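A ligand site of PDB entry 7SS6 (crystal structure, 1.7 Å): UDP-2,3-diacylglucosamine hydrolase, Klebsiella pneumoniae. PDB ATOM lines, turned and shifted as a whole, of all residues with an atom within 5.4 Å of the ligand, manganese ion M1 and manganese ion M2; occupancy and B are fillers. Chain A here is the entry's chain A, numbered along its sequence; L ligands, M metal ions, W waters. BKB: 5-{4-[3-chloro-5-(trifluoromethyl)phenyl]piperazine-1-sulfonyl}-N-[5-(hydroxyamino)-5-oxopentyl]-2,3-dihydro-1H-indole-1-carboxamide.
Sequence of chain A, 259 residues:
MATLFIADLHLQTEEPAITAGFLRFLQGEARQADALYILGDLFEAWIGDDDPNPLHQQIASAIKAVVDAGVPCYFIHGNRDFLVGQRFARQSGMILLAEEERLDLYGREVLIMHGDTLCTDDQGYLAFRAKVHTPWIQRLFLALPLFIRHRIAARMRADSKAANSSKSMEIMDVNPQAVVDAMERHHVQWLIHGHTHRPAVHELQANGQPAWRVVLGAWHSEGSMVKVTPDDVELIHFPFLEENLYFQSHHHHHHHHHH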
ATOM      1  N   ASP A   8     -15.267 -20.212 -38.382  1.00  0.00           N
ATOM      2  CA  ASP A   8     -16.302 -19.453 -37.713  1.00  0.00           C
ATOM      3  C   ASP A   8     -17.575 -20.262 -37.500  1.00  0.00           C
ATOM      4  O   ASP A   8     -18.689 -19.777 -37.702  1.00  0.00           O
ATOM      5  CB  ASP A   8     -16.577 -18.171 -38.497  1.00  0.00           C
ATOM      6  CG  ASP A   8     -15.355 -17.273 -38.529  1.00  0.00           C
ATOM      7  OD1 ASP A   8     -14.946 -16.853 -37.440  1.00  0.00           O
ATOM      8  OD2 ASP A   8     -14.813 -16.990 -39.611  1.00  0.00           O
ATOM      9  N   HIS A  10     -18.086 -21.525 -34.363  1.00  0.00           N
ATOM     10  CA  HIS A  10     -18.374 -21.119 -32.976  1.00  0.00           C
ATOM     11  C   HIS A  10     -19.197 -22.185 -32.251  1.00  0.00           C
ATOM     12  O   HIS A  10     -20.211 -21.892 -31.620  1.00  0.00           O
ATOM     13  CB  HIS A  10     -19.093 -19.762 -32.948  1.00  0.00           C
ATOM     14  CG  HIS A  10     -18.485 -18.745 -33.856  1.00  0.00           C
ATOM     15  ND1 HIS A  10     -19.092 -18.316 -35.011  1.00  0.00           N
ATOM     16  CD2 HIS A  10     -17.306 -18.076 -33.780  1.00  0.00           C
ATOM     17  CE1 HIS A  10     -18.322 -17.438 -35.621  1.00  0.00           C
ATOM     18  NE2 HIS A  10     -17.227 -17.281 -34.893  1.00  0.00           N
ATOM     19  N   ASP A  41     -11.765 -20.372 -35.105  1.00  0.00           N
ATOM     20  CA  ASP A  41     -13.093 -20.201 -34.496  1.00  0.00           C
ATOM     21  C   ASP A  41     -13.976 -21.407 -34.787  1.00  0.00           C
ATOM     22  O   ASP A  41     -15.180 -21.301 -35.053  1.00  0.00           O
ATOM     23  CB  ASP A  41     -13.757 -18.898 -34.957  1.00  0.00           C
ATOM     24  CG  ASP A  41     -13.097 -17.655 -34.378  1.00  0.00           C
ATOM     25  OD1 ASP A  41     -12.160 -17.782 -33.571  1.00  0.00           O
ATOM     26  OD2 ASP A  41     -13.541 -16.563 -34.735  1.00  0.00           O
ATOM     27  N   GLU A  44     -16.590 -21.802 -29.908  1.00  0.00           N
ATOM     28  CA  GLU A  44     -16.885 -20.460 -29.410  1.00  0.00           C
ATOM     29  C   GLU A  44     -15.949 -20.060 -28.285  1.00  0.00           C
ATOM     30  O   GLU A  44     -15.728 -18.861 -28.050  1.00  0.00           O
ATOM     31  CB  GLU A  44     -18.348 -20.407 -28.943  1.00  0.00           C
ATOM     32  CG  GLU A  44     -18.755 -19.117 -28.184  1.00  0.00           C
ATOM     33  CD  GLU A  44     -18.786 -17.846 -29.024  1.00  0.00           C
ATOM     34  OE1 GLU A  44     -18.403 -17.866 -30.203  1.00  0.00           O
ATOM     35  OE2 GLU A  44     -19.181 -16.793 -28.466  1.00  0.00           O
ATOM     36  N   ALA A  45     -15.376 -21.040 -27.589  1.00  0.00           N
ATOM     37  CA  ALA A  45     -14.461 -20.778 -26.494  1.00  0.00           C
ATOM     38  C   ALA A  45     -13.516 -21.962 -26.361  1.00  0.00           C
ATOM     39  O   ALA A  45     -13.860 -23.077 -26.743  1.00  0.00           O
ATOM     40  CB  ALA A  45     -15.233 -20.561 -25.178  1.00  0.00           C
ATOM     41  N   TRP A  46     -12.324 -21.715 -25.807  1.00  0.00           N
ATOM     42  CA  TRP A  46     -11.422 -22.802 -25.449  1.00  0.00           C
ATOM     43  C   TRP A  46     -10.572 -22.331 -24.276  1.00  0.00           C
ATOM     44  O   TRP A  46      -9.982 -21.259 -24.332  1.00  0.00           O
ATOM     45  CB  TRP A  46     -10.492 -23.188 -26.607  1.00  0.00           C
ATOM     46  CG  TRP A  46      -9.924 -24.599 -26.520  1.00  0.00           C
ATOM     47  CD1 TRP A  46      -8.693 -24.976 -26.049  1.00  0.00           C
ATOM     48  CD2 TRP A  46     -10.578 -25.805 -26.949  1.00  0.00           C
ATOM     49  NE1 TRP A  46      -8.549 -26.358 -26.160  1.00  0.00           N
ATOM     50  CE2 TRP A  46      -9.697 -26.877 -26.702  1.00  0.00           C
ATOM     51  CE3 TRP A  46     -11.833 -26.072 -27.516  1.00  0.00           C
ATOM     52  CZ2 TRP A  46     -10.024 -28.206 -27.036  1.00  0.00           C
ATOM     53  CZ3 TRP A  46     -12.157 -27.403 -27.837  1.00  0.00           C
ATOM     54  CH2 TRP A  46     -11.249 -28.437 -27.596  1.00  0.00           C
ATOM     55  N   ILE A  47     -10.519 -23.145 -23.220  1.00  0.00           N
ATOM     56  CA  ILE A  47      -9.695 -22.823 -22.055  1.00  0.00           C
ATOM     57  C   ILE A  47      -8.606 -23.861 -21.828  1.00  0.00           C
ATOM     58  O   ILE A  47      -7.911 -23.812 -20.814  1.00  0.00           O
ATOM     59  CB  ILE A  47     -10.556 -22.630 -20.784  1.00  0.00           C
ATOM     60  CG1 ILE A  47     -11.338 -23.908 -20.437  1.00  0.00           C
ATOM     61  CG2 ILE A  47     -11.476 -21.421 -20.940  1.00  0.00           C
ATOM     62  CD1 ILE A  47     -12.084 -23.820 -19.114  1.00  0.00           C
ATOM     63  N   GLY A  78      -8.286 -19.644 -34.362  1.00  0.00           N
ATOM     64  CA  GLY A  78      -9.013 -18.385 -34.345  1.00  0.00           C
ATOM     65  C   GLY A  78      -8.752 -17.638 -33.053  1.00  0.00           C
ATOM     66  O   GLY A  78      -8.050 -18.108 -32.160  1.00  0.00           O
ATOM     67  N   ASN A  79      -9.347 -16.454 -32.947  1.00  0.00           N
ATOM     68  CA  ASN A  79      -9.259 -15.701 -31.709  1.00  0.00           C
ATOM     69  C   ASN A  79     -10.131 -16.292 -30.606  1.00  0.00           C
ATOM     70  O   ASN A  79      -9.873 -16.035 -29.430  1.00  0.00           O
ATOM     71  CB  ASN A  79      -9.643 -14.246 -31.948  1.00  0.00           C
ATOM     72  CG  ASN A  79     -11.026 -14.107 -32.516  1.00  0.00           C
ATOM     73  OD1 ASN A  79     -11.275 -14.482 -33.666  1.00  0.00           O
ATOM     74  ND2 ASN A  79     -11.941 -13.548 -31.737  1.00  0.00           N
ATOM     75  N   ARG A  80     -11.164 -17.077 -30.958  1.00  0.00           N
ATOM     76  CA  ARG A  80     -11.955 -17.715 -29.920  1.00  0.00           C
ATOM     77  C   ARG A  80     -11.266 -18.959 -29.369  1.00  0.00           C
ATOM     78  O   ARG A  80     -11.430 -19.281 -28.176  1.00  0.00           O
ATOM     79  CB  ARG A  80     -13.349 -18.097 -30.440  1.00  0.00           C
ATOM     80  CG  ARG A  80     -14.159 -16.966 -31.063  1.00  0.00           C
ATOM     81  CD  ARG A  80     -14.403 -15.829 -30.058  1.00  0.00           C
ATOM     82  NE  ARG A  80     -15.170 -16.289 -28.907  1.00  0.00           N
ATOM     83  CZ  ARG A  80     -15.786 -15.485 -28.057  1.00  0.00           C
ATOM     84  NH1 ARG A  80     -15.808 -14.169 -28.232  1.00  0.00           N
ATOM     85  NH2 ARG A  80     -16.406 -16.002 -27.000  1.00  0.00           N
ATOM     86  N   PHE A  82      -7.777 -20.004 -29.650  1.00  0.00           N
ATOM     87  CA  PHE A  82      -6.327 -20.002 -29.787  1.00  0.00           C
ATOM     88  C   PHE A  82      -5.630 -20.942 -28.797  1.00  0.00           C
ATOM     89  O   PHE A  82      -4.454 -21.264 -28.999  1.00  0.00           O
ATOM     90  CB  PHE A  82      -5.760 -18.576 -29.617  1.00  0.00           C
ATOM     91  CG  PHE A  82      -6.047 -17.934 -28.285  1.00  0.00           C
ATOM     92  CD1 PHE A  82      -7.227 -17.221 -28.081  1.00  0.00           C
ATOM     93  CD2 PHE A  82      -5.145 -18.046 -27.230  1.00  0.00           C
ATOM     94  CE1 PHE A  82      -7.500 -16.622 -26.845  1.00  0.00           C
ATOM     95  CE2 PHE A  82      -5.419 -17.453 -26.002  1.00  0.00           C
ATOM     96  CZ  PHE A  82      -6.602 -16.752 -25.814  1.00  0.00           C
ATOM     97  N   LEU A  83      -6.330 -21.432 -27.786  1.00  0.00           N
ATOM     98  CA  LEU A  83      -5.695 -22.365 -26.856  1.00  0.00           C
ATOM     99  C   LEU A  83      -5.829 -23.823 -27.274  1.00  0.00           C
ATOM    100  O   LEU A  83      -5.362 -24.697 -26.528  1.00  0.00           O
ATOM    101  CB  LEU A  83      -6.274 -22.188 -25.437  1.00  0.00           C
ATOM    102  CG  LEU A  83      -5.901 -20.872 -24.744  1.00  0.00           C
ATOM    103  CD1 LEU A  83      -6.524 -20.811 -23.368  1.00  0.00           C
ATOM    104  CD2 LEU A  83      -4.371 -20.730 -24.645  1.00  0.00           C
ATOM    105  N   HIS A 114      -6.724 -17.071 -40.295  1.00  0.00           N
ATOM    106  CA  HIS A 114      -8.027 -16.827 -39.696  1.00  0.00           C
ATOM    107  C   HIS A 114      -8.582 -15.485 -40.165  1.00  0.00           C
ATOM    108  O   HIS A 114      -9.773 -15.358 -40.473  1.00  0.00           O
ATOM    109  CB  HIS A 114      -7.968 -16.849 -38.171  1.00  0.00           C
ATOM    110  CG  HIS A 114      -9.293 -16.618 -37.532  1.00  0.00           C
ATOM    111  ND1 HIS A 114     -10.390 -17.410 -37.793  1.00  0.00           N
ATOM    112  CD2 HIS A 114      -9.735 -15.640 -36.692  1.00  0.00           C
ATOM    113  CE1 HIS A 114     -11.433 -16.966 -37.121  1.00  0.00           C
ATOM    114  NE2 HIS A 114     -11.064 -15.890 -36.444  1.00  0.00           N
ATOM    115  N   ASP A 116      -8.018 -12.379 -38.403  1.00  0.00           N
ATOM    116  CA  ASP A 116      -8.042 -11.285 -37.424  1.00  0.00           C
ATOM    117  C   ASP A 116      -6.779 -10.436 -37.462  1.00  0.00           C
ATOM    118  O   ASP A 116      -6.824  -9.240 -37.133  1.00  0.00           O
ATOM    119  CB  ASP A 116      -8.257 -11.825 -36.003  1.00  0.00           C
ATOM    120  CG  ASP A 116      -7.205 -12.839 -35.584  1.00  0.00           C
ATOM    121  OD1 ASP A 116      -6.913 -13.788 -36.348  1.00  0.00           O
ATOM    122  OD2 ASP A 116      -6.695 -12.710 -34.451  1.00  0.00           O
ATOM    123  N   TYR A 125      -7.659  -4.439 -30.093  1.00  0.00           N
ATOM    124  CA  TYR A 125      -7.751  -5.892 -30.228  1.00  0.00           C
ATOM    125  C   TYR A 125      -6.371  -6.510 -30.435  1.00  0.00           C
ATOM    126  O   TYR A 125      -6.009  -7.494 -29.779  1.00  0.00           O
ATOM    127  CB  TYR A 125      -8.682  -6.261 -31.378  1.00  0.00           C
ATOM    128  CG  TYR A 125      -8.534  -7.727 -31.705  1.00  0.00           C
ATOM    129  CD1 TYR A 125      -8.952  -8.677 -30.802  1.00  0.00           C
ATOM    130  CD2 TYR A 125      -7.909  -8.131 -32.865  1.00  0.00           C
ATOM    131  CE1 TYR A 125      -8.797 -10.023 -31.070  1.00  0.00           C
ATOM    132  CE2 TYR A 125      -7.746  -9.483 -33.143  1.00  0.00           C
ATOM    133  CZ  TYR A 125      -8.193 -10.420 -32.233  1.00  0.00           C
ATOM    134  OH  TYR A 125      -8.046 -11.754 -32.483  1.00  0.00           O
ATOM    135  N   PHE A 128      -4.359  -6.804 -27.154  1.00  0.00           N
ATOM    136  CA  PHE A 128      -4.855  -7.944 -26.385  1.00  0.00           C
ATOM    137  C   PHE A 128      -4.457  -9.270 -27.038  1.00  0.00           C
ATOM    138  O   PHE A 128      -4.061 -10.214 -26.355  1.00  0.00           O
ATOM    139  CB  PHE A 128      -6.373  -7.858 -26.267  1.00  0.00           C
ATOM    140  CG  PHE A 128      -7.019  -9.124 -25.784  1.00  0.00           C
ATOM    141  CD1 PHE A 128      -6.942  -9.505 -24.456  1.00  0.00           C
ATOM    142  CD2 PHE A 128      -7.703  -9.953 -26.680  1.00  0.00           C
ATOM    143  CE1 PHE A 128      -7.541 -10.677 -24.028  1.00  0.00           C
ATOM    144  CE2 PHE A 128      -8.292 -11.125 -26.254  1.00  0.00           C
ATOM    145  CZ  PHE A 128      -8.215 -11.491 -24.924  1.00  0.00           C
ATOM    146  N   VAL A 132      -2.383 -12.495 -25.180  1.00  0.00           N
ATOM    147  CA  VAL A 132      -2.798 -13.886 -25.019  1.00  0.00           C
ATOM    148  C   VAL A 132      -2.056 -14.843 -25.935  1.00  0.00           C
ATOM    149  O   VAL A 132      -2.234 -16.052 -25.824  1.00  0.00           O
ATOM    150  CB  VAL A 132      -4.314 -14.091 -25.223  1.00  0.00           C
ATOM    151  CG1 VAL A 132      -5.110 -13.294 -24.188  1.00  0.00           C
ATOM    152  CG2 VAL A 132      -4.736 -13.742 -26.664  1.00  0.00           C
ATOM    153  N   ILE A 137       2.374 -16.118 -20.843  1.00  0.00           N
ATOM    154  CA  ILE A 137       1.020 -15.838 -20.402  1.00  0.00           C
ATOM    155  C   ILE A 137       0.117 -17.045 -20.640  1.00  0.00           C
ATOM    156  O   ILE A 137      -0.664 -17.425 -19.765  1.00  0.00           O
ATOM    157  CB  ILE A 137       0.500 -14.560 -21.083  1.00  0.00           C
ATOM    158  CG1 ILE A 137       1.337 -13.359 -20.652  1.00  0.00           C
ATOM    159  CG2 ILE A 137      -0.966 -14.324 -20.758  1.00  0.00           C
ATOM    160  CD1 ILE A 137       0.902 -12.041 -21.249  1.00  0.00           C
ATOM    161  N   GLN A 138       0.207 -17.674 -21.823  1.00  0.00           N
ATOM    162  CA  GLN A 138      -0.585 -18.887 -22.061  1.00  0.00           C
ATOM    163  C   GLN A 138      -0.255 -19.977 -21.050  1.00  0.00           C
ATOM    164  O   GLN A 138      -1.162 -20.651 -20.540  1.00  0.00           O
ATOM    165  CB  GLN A 138      -0.348 -19.411 -23.476  1.00  0.00           C
ATOM    166  CG  GLN A 138      -0.877 -18.521 -24.555  1.00  0.00           C
ATOM    167  CD  GLN A 138      -0.910 -19.233 -25.871  1.00  0.00           C
ATOM    168  OE1 GLN A 138      -0.458 -20.377 -25.973  1.00  0.00           O
ATOM    169  NE2 GLN A 138      -1.450 -18.580 -26.893  1.00  0.00           N
ATOM    170  N   PHE A 141      -1.891 -19.188 -17.685  1.00  0.00           N
ATOM    171  CA  PHE A 141      -3.342 -19.411 -17.708  1.00  0.00           C
ATOM    172  C   PHE A 141      -3.660 -20.894 -17.644  1.00  0.00           C
ATOM    173  O   PHE A 141      -4.507 -21.332 -16.866  1.00  0.00           O
ATOM    174  CB  PHE A 141      -3.955 -18.782 -18.966  1.00  0.00           C
ATOM    175  CG  PHE A 141      -5.444 -19.007 -19.084  1.00  0.00           C
ATOM    176  CD1 PHE A 141      -6.342 -18.172 -18.431  1.00  0.00           C
ATOM    177  CD2 PHE A 141      -5.945 -20.042 -19.861  1.00  0.00           C
ATOM    178  CE1 PHE A 141      -7.712 -18.372 -18.560  1.00  0.00           C
ATOM    179  CE2 PHE A 141      -7.310 -20.245 -19.963  1.00  0.00           C
ATOM    180  CZ  PHE A 141      -8.190 -19.422 -19.329  1.00  0.00           C
ATOM    181  N   ILE A 152     -13.028 -17.527 -15.215  1.00  0.00           N
ATOM    182  CA  ILE A 152     -12.415 -16.383 -15.903  1.00  0.00           C
ATOM    183  C   ILE A 152     -13.062 -16.211 -17.275  1.00  0.00           C
ATOM    184  O   ILE A 152     -13.499 -15.123 -17.655  1.00  0.00           O
ATOM    185  CB  ILE A 152     -10.897 -16.559 -16.041  1.00  0.00           C
ATOM    186  CG1 ILE A 152     -10.195 -16.393 -14.686  1.00  0.00           C
ATOM    187  CG2 ILE A 152     -10.331 -15.590 -17.071  1.00  0.00           C
ATOM    188  CD1 ILE A 152      -8.741 -16.825 -14.730  1.00  0.00           C
ATOM    189  N   ALA A 153     -13.166 -17.325 -18.014  1.00  0.00           N
ATOM    190  CA  ALA A 153     -13.686 -17.266 -19.381  1.00  0.00           C
ATOM    191  C   ALA A 153     -15.150 -16.840 -19.394  1.00  0.00           C
ATOM    192  O   ALA A 153     -15.551 -16.030 -20.240  1.00  0.00           O
ATOM    193  CB  ALA A 153     -13.505 -18.620 -20.055  1.00  0.00           C
ATOM    194  N   ALA A 154     -15.956 -17.377 -18.471  1.00  0.00           N
ATOM    195  CA  ALA A 154     -17.369 -17.013 -18.444  1.00  0.00           C
ATOM    196  C   ALA A 154     -17.548 -15.540 -18.117  1.00  0.00           C
ATOM    197  O   ALA A 154     -18.407 -14.862 -18.713  1.00  0.00           O
ATOM    198  CB  ALA A 154     -18.127 -17.881 -17.436  1.00  0.00           C
ATOM    199  N   MET A 156     -15.314 -13.161 -18.753  1.00  0.00           N
ATOM    200  CA  MET A 156     -14.826 -12.438 -19.925  1.00  0.00           C
ATOM    201  C   MET A 156     -15.867 -12.421 -21.038  1.00  0.00           C
ATOM    202  O   MET A 156     -16.070 -11.390 -21.703  1.00  0.00           O
ATOM    203  CB  MET A 156     -13.533 -13.114 -20.392  1.00  0.00           C
ATOM    204  CG  MET A 156     -12.394 -12.905 -19.418  1.00  0.00           C
ATOM    205  SD  MET A 156     -10.739 -13.127 -20.090  1.00  0.00           S
ATOM    206  CE  MET A 156     -10.895 -12.406 -21.720  1.00  0.00           C
ATOM    207  N   ARG A 157     -16.528 -13.554 -21.268  1.00  0.00           N
ATOM    208  CA  ARG A 157     -17.586 -13.609 -22.272  1.00  0.00           C
ATOM    209  C   ARG A 157     -18.782 -12.761 -21.851  1.00  0.00           C
ATOM    210  O   ARG A 157     -19.370 -12.048 -22.682  1.00  0.00           O
ATOM    211  CB  ARG A 157     -18.007 -15.049 -22.531  1.00  0.00           C
ATOM    212  CG  ARG A 157     -16.933 -15.896 -23.227  1.00  0.00           C
ATOM    213  CD  ARG A 157     -17.500 -17.223 -23.704  1.00  0.00           C
ATOM    214  NE  ARG A 157     -18.049 -18.009 -22.601  1.00  0.00           N
ATOM    215  CZ  ARG A 157     -17.341 -18.858 -21.862  1.00  0.00           C
ATOM    216  NH1 ARG A 157     -16.062 -19.081 -22.092  1.00  0.00           N
ATOM    217  NH2 ARG A 157     -17.947 -19.508 -20.869  1.00  0.00           N
ATOM    218  N   SER A 160     -17.837  -9.150 -22.489  1.00  0.00           N
ATOM    219  CA  SER A 160     -17.734  -8.736 -23.884  1.00  0.00           C
ATOM    220  C   SER A 160     -19.104  -8.606 -24.550  1.00  0.00           C
ATOM    221  O   SER A 160     -19.258  -7.829 -25.498  1.00  0.00           O
ATOM    222  CB  SER A 160     -16.865  -9.710 -24.666  1.00  0.00           C
ATOM    223  OG  SER A 160     -15.489  -9.502 -24.392  1.00  0.00           O
ATOM    224  N   ILE A 171     -18.094  -6.542 -35.993  1.00  0.00           N
ATOM    225  CA  ILE A 171     -16.697  -6.943 -36.117  1.00  0.00           C
ATOM    226  C   ILE A 171     -15.973  -6.003 -37.072  1.00  0.00           C
ATOM    227  O   ILE A 171     -16.426  -5.769 -38.203  1.00  0.00           O
ATOM    228  CB  ILE A 171     -16.595  -8.406 -36.580  1.00  0.00           C
ATOM    229  CG1 ILE A 171     -17.548  -9.294 -35.755  1.00  0.00           C
ATOM    230  CG2 ILE A 171     -15.143  -8.900 -36.588  1.00  0.00           C
ATOM    231  CD1 ILE A 171     -17.561 -10.749 -36.181  1.00  0.00           C
ATOM    232  N   HIS A 195     -13.100 -14.905 -39.823  1.00  0.00           N
ATOM    233  CA  HIS A 195     -13.101 -13.868 -38.791  1.00  0.00           C
ATOM    234  C   HIS A 195     -14.090 -12.724 -39.001  1.00  0.00           C
ATOM    235  O   HIS A 195     -14.792 -12.350 -38.047  1.00  0.00           O
ATOM    236  CB  HIS A 195     -11.714 -13.277 -38.598  1.00  0.00           C
ATOM    237  CG  HIS A 195     -11.649 -12.314 -37.442  1.00  0.00           C
ATOM    238  ND1 HIS A 195     -11.799 -12.709 -36.131  1.00  0.00           N
ATOM    239  CD2 HIS A 195     -11.479 -10.968 -37.403  1.00  0.00           C
ATOM    240  CE1 HIS A 195     -11.711 -11.654 -35.331  1.00  0.00           C
ATOM    241  NE2 HIS A 195     -11.516 -10.585 -36.088  1.00  0.00           N
ATOM    242  N   THR A 196     -14.150 -12.141 -40.196  1.00  0.00           N
ATOM    243  CA  THR A 196     -14.979 -10.950 -40.365  1.00  0.00           C
ATOM    244  C   THR A 196     -16.452 -11.268 -40.527  1.00  0.00           C
ATOM    245  O   THR A 196     -17.282 -10.358 -40.479  1.00  0.00           O
ATOM    246  CB  THR A 196     -14.497 -10.125 -41.551  1.00  0.00           C
ATOM    247  OG1 THR A 196     -14.641 -10.904 -42.761  1.00  0.00           O
ATOM    248  CG2 THR A 196     -13.023  -9.725 -41.364  1.00  0.00           C
ATOM    249  N   HIS A 197     -16.811 -12.542 -40.746  1.00  0.00           N
ATOM    250  CA  HIS A 197     -18.197 -12.988 -40.848  1.00  0.00           C
ATOM    251  C   HIS A 197     -18.934 -12.299 -41.994  1.00  0.00           C
ATOM    252  O   HIS A 197     -20.150 -12.081 -41.923  1.00  0.00           O
ATOM    253  CB  HIS A 197     -18.940 -12.770 -39.537  1.00  0.00           C
ATOM    254  CG  HIS A 197     -18.379 -13.557 -38.377  1.00  0.00           C
ATOM    255  ND1 HIS A 197     -18.995 -13.577 -37.145  1.00  0.00           N
ATOM    256  CD2 HIS A 197     -17.293 -14.349 -38.276  1.00  0.00           C
ATOM    257  CE1 HIS A 197     -18.296 -14.357 -36.330  1.00  0.00           C
ATOM    258  NE2 HIS A 197     -17.248 -14.819 -36.976  1.00  0.00           N
HETATM  259  C13 BKB L   1     -12.168 -16.123 -26.341  1.00  0.00           C
HETATM  260  C15 BKB L   1     -12.951 -13.858 -26.534  1.00  0.00           C
HETATM  261  C17 BKB L   1     -13.471 -15.080 -24.537  1.00  0.00           C
HETATM  262  C21 BKB L   1     -12.897 -12.164 -28.480  1.00  0.00           C
HETATM  263  C24 BKB L   1     -12.937 -10.429 -30.316  1.00  0.00           C
HETATM  264  C26 BKB L   1     -13.972 -10.601 -32.647  1.00  0.00           C
HETATM  265  C28 BKB L   1     -14.605 -12.587 -34.057  1.00  0.00           C
HETATM  266  C01 BKB L   1      -6.438 -16.810 -22.135  1.00  0.00           C
HETATM  267  C02 BKB L   1      -7.592 -16.277 -21.605  1.00  0.00           C
HETATM  268  C04 BKB L   1     -10.057 -16.656 -21.311  1.00  0.00           C
HETATM  269  C05 BKB L   1     -11.211 -16.404 -22.270  1.00  0.00           C
HETATM  270  C07 BKB L   1     -10.060 -17.664 -23.957  1.00  0.00           C
HETATM  271  C08 BKB L   1      -8.850 -17.856 -23.066  1.00  0.00           C
HETATM  272  C12 BKB L   1     -12.791 -16.145 -25.093  1.00  0.00           C
HETATM  273  C14 BKB L   1     -12.259 -14.958 -27.089  1.00  0.00           C
HETATM  274  C16 BKB L   1     -13.563 -13.902 -25.284  1.00  0.00           C
HETATM  275  C18 BKB L   1     -14.239 -12.568 -24.976  1.00  0.00           C
HETATM  276  C19 BKB L   1     -13.878 -11.675 -26.144  1.00  0.00           C
HETATM  277  C25 BKB L   1     -14.098 -11.027 -31.163  1.00  0.00           C
HETATM  278  C27 BKB L   1     -15.084 -11.240 -33.509  1.00  0.00           C
HETATM  279  C32 BKB L   1      -7.586 -15.314 -20.605  1.00  0.00           C
HETATM  280  C33 BKB L   1      -6.368 -14.869 -20.146  1.00  0.00           C
HETATM  281  C34 BKB L   1      -5.183 -15.361 -20.662  1.00  0.00           C
HETATM  282  C35 BKB L   1      -5.231 -16.330 -21.676  1.00  0.00           C
HETATM  283  C37 BKB L   1      -6.367 -13.806 -19.045  1.00  0.00           C
HETATM  284  F38 BKB L   1      -7.082 -12.747 -19.500  1.00  0.00           F
HETATM  285  F39 BKB L   1      -5.084 -13.445 -18.797  1.00  0.00           F
HETATM  286  F40 BKB L   1      -6.947 -14.287 -17.932  1.00  0.00           F
HETATM  287  N03 BKB L   1      -8.845 -16.754 -22.099  1.00  0.00           N
HETATM  288  N06 BKB L   1     -11.284 -17.551 -23.179  1.00  0.00           N
HETATM  289  N20 BKB L   1     -13.212 -12.526 -27.118  1.00  0.00           N
HETATM  290  N23 BKB L   1     -13.236 -10.808 -28.930  1.00  0.00           N
HETATM  291  N30 BKB L   1     -14.894 -12.981 -35.427  1.00  0.00           N
HETATM  292  O10 BKB L   1     -13.880 -17.728 -23.276  1.00  0.00           O
HETATM  293  O11 BKB L   1     -12.569 -18.804 -24.991  1.00  0.00           O
HETATM  294  O22 BKB L   1     -12.358 -12.938 -29.188  1.00  0.00           O
HETATM  295  O29 BKB L   1     -13.975 -13.354 -33.394  1.00  0.00           O
HETATM  296  O31 BKB L   1     -14.409 -14.242 -35.812  1.00  0.00           O
HETATM  297  S09 BKB L   1     -12.694 -17.635 -24.106  1.00  0.00           S
HETATM  298 CL36 BKB L   1      -3.745 -16.981 -22.358  1.00  0.00          CL
HETATM  299 MN    MN M   1     -15.646 -15.930 -35.752  1.00  0.00          MN
HETATM  300 MN    MN M   2     -12.525 -14.704 -35.186  1.00  0.00          MN
HETATM  301  O   HOH W   1     -16.066 -14.933 -33.579  1.00  0.00           O
HETATM  302  O   HOH W   2     -16.650 -13.243 -31.382  1.00  0.00           O
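Manganese ion M2 is bound by OD1 of Asn 79 (2.0 Å), O31 of the ligand (2.0 Å), OD2 of Asp 41 (2.2 Å), NE2 of His 114 (2.3 Å), ND1 of His 195 (2.3 Å) and O29 of the ligand (2.7 Å).
Manganese ion M2 has six donor atoms within binding distance.
Four residues have an atom within 4 Å of manganese ion M1: Asp 8, His 10, Asp 41 and His 197.
OD1 of Asp 41 lies within hydrogen-bond range of N of Arg 80, at 2.9 Å.
OD2 of Asp 8 is in hydrogen-bond range of N of His 195.
The guanidinium group (NH2) of Arg 80 lies within salt-bridge range of the side-chain carboxylate (OE2) of Glu 44 (3.2 Å).
The backbone carbonyl oxygen (O) of Met 156 sits at hydrogen-bond distance from the side-chain hydroxyl (OG) of Ser 160, 3.3 Å away.
O of Val 132 lies within hydrogen-bond range of NE2 of Gln 138 (2.9 Å).
Along chain A the residues within 4 Å of manganese ion M2 span positions 8 to 195.
The nearest printed residue that does not touch manganese ion M2 is Arg 80 (5.0 Å).
O10 of the ligand is in hydrogen-bond range of NH1 of Arg 157 (2.8 Å).
The backbone carbonyl oxygen of His 195 is in hydrogen-bond range of a nitrogen (N30) of the ligand.
The backbone NH (N) of Trp 46 sits at hydrogen-bond distance from an oxygen (O11) of the ligand (3.0 Å).
Manganese ion M1 is bound by OD1 of Asp 8 (2.0 Å), O31 of the ligand (2.1 Å), NE2 of His 10 (2.3 Å), NE2 of His 197 (2.3 Å), OD2 of Asp 41 (2.4 Å) and water W1 (2.4 Å).
The guanidinium group (NH1) of Arg 80 lies close to a nitrogen (N20) of the ligand (3.3 Å).
The side-chain sulfur of Met 156 sits close to a fluorine (F38) of the ligand (3.7 Å).
Ala 45 touches the ligand.
CZ of Phe 82 touches C01 of the ligand (3.7 Å).
Leu 83 touches the ligand (CD1 to C08, 3.8 Å).
O of Val 132 touches CL36 of the ligand (3.9 Å).
CA of Gln 138 touches CL36 of the ligand, 3.7 Å away.
CE1 of Phe 141 touches C32 of the ligand, 3.7 Å away.
CG2 of Ile 152 touches F40 of the ligand (3.7 Å).
CB of Ala 153 touches O10 of the ligand (3.4 Å).
OG of Ser 160 touches C19 of the ligand (3.2 Å).
CD1 of Ile 171 touches N30 of the ligand (3.6 Å).
Hydrophobic or aromatic side chains within 4 Å of the ligand: Ala 45, Phe 82, Leu 83, Val 132, Phe 141, Ile 152, Ala 153, Met 156, Ile 171, His 195 and His 197.
Within 4 Å of the ligand: Asp 8, Asp 41, Ala 45, Trp 46, Asn 79, Arg 80, Phe 82, Leu 83, His 114, Val 132, Gln 138, Phe 141, Ile 152, Ala 153, Met 156, Arg 157, Ser 160, Ile 171, His 195 and His 197.
Along chain A the residues within 4 Å of the ligand span positions 8 to 197.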
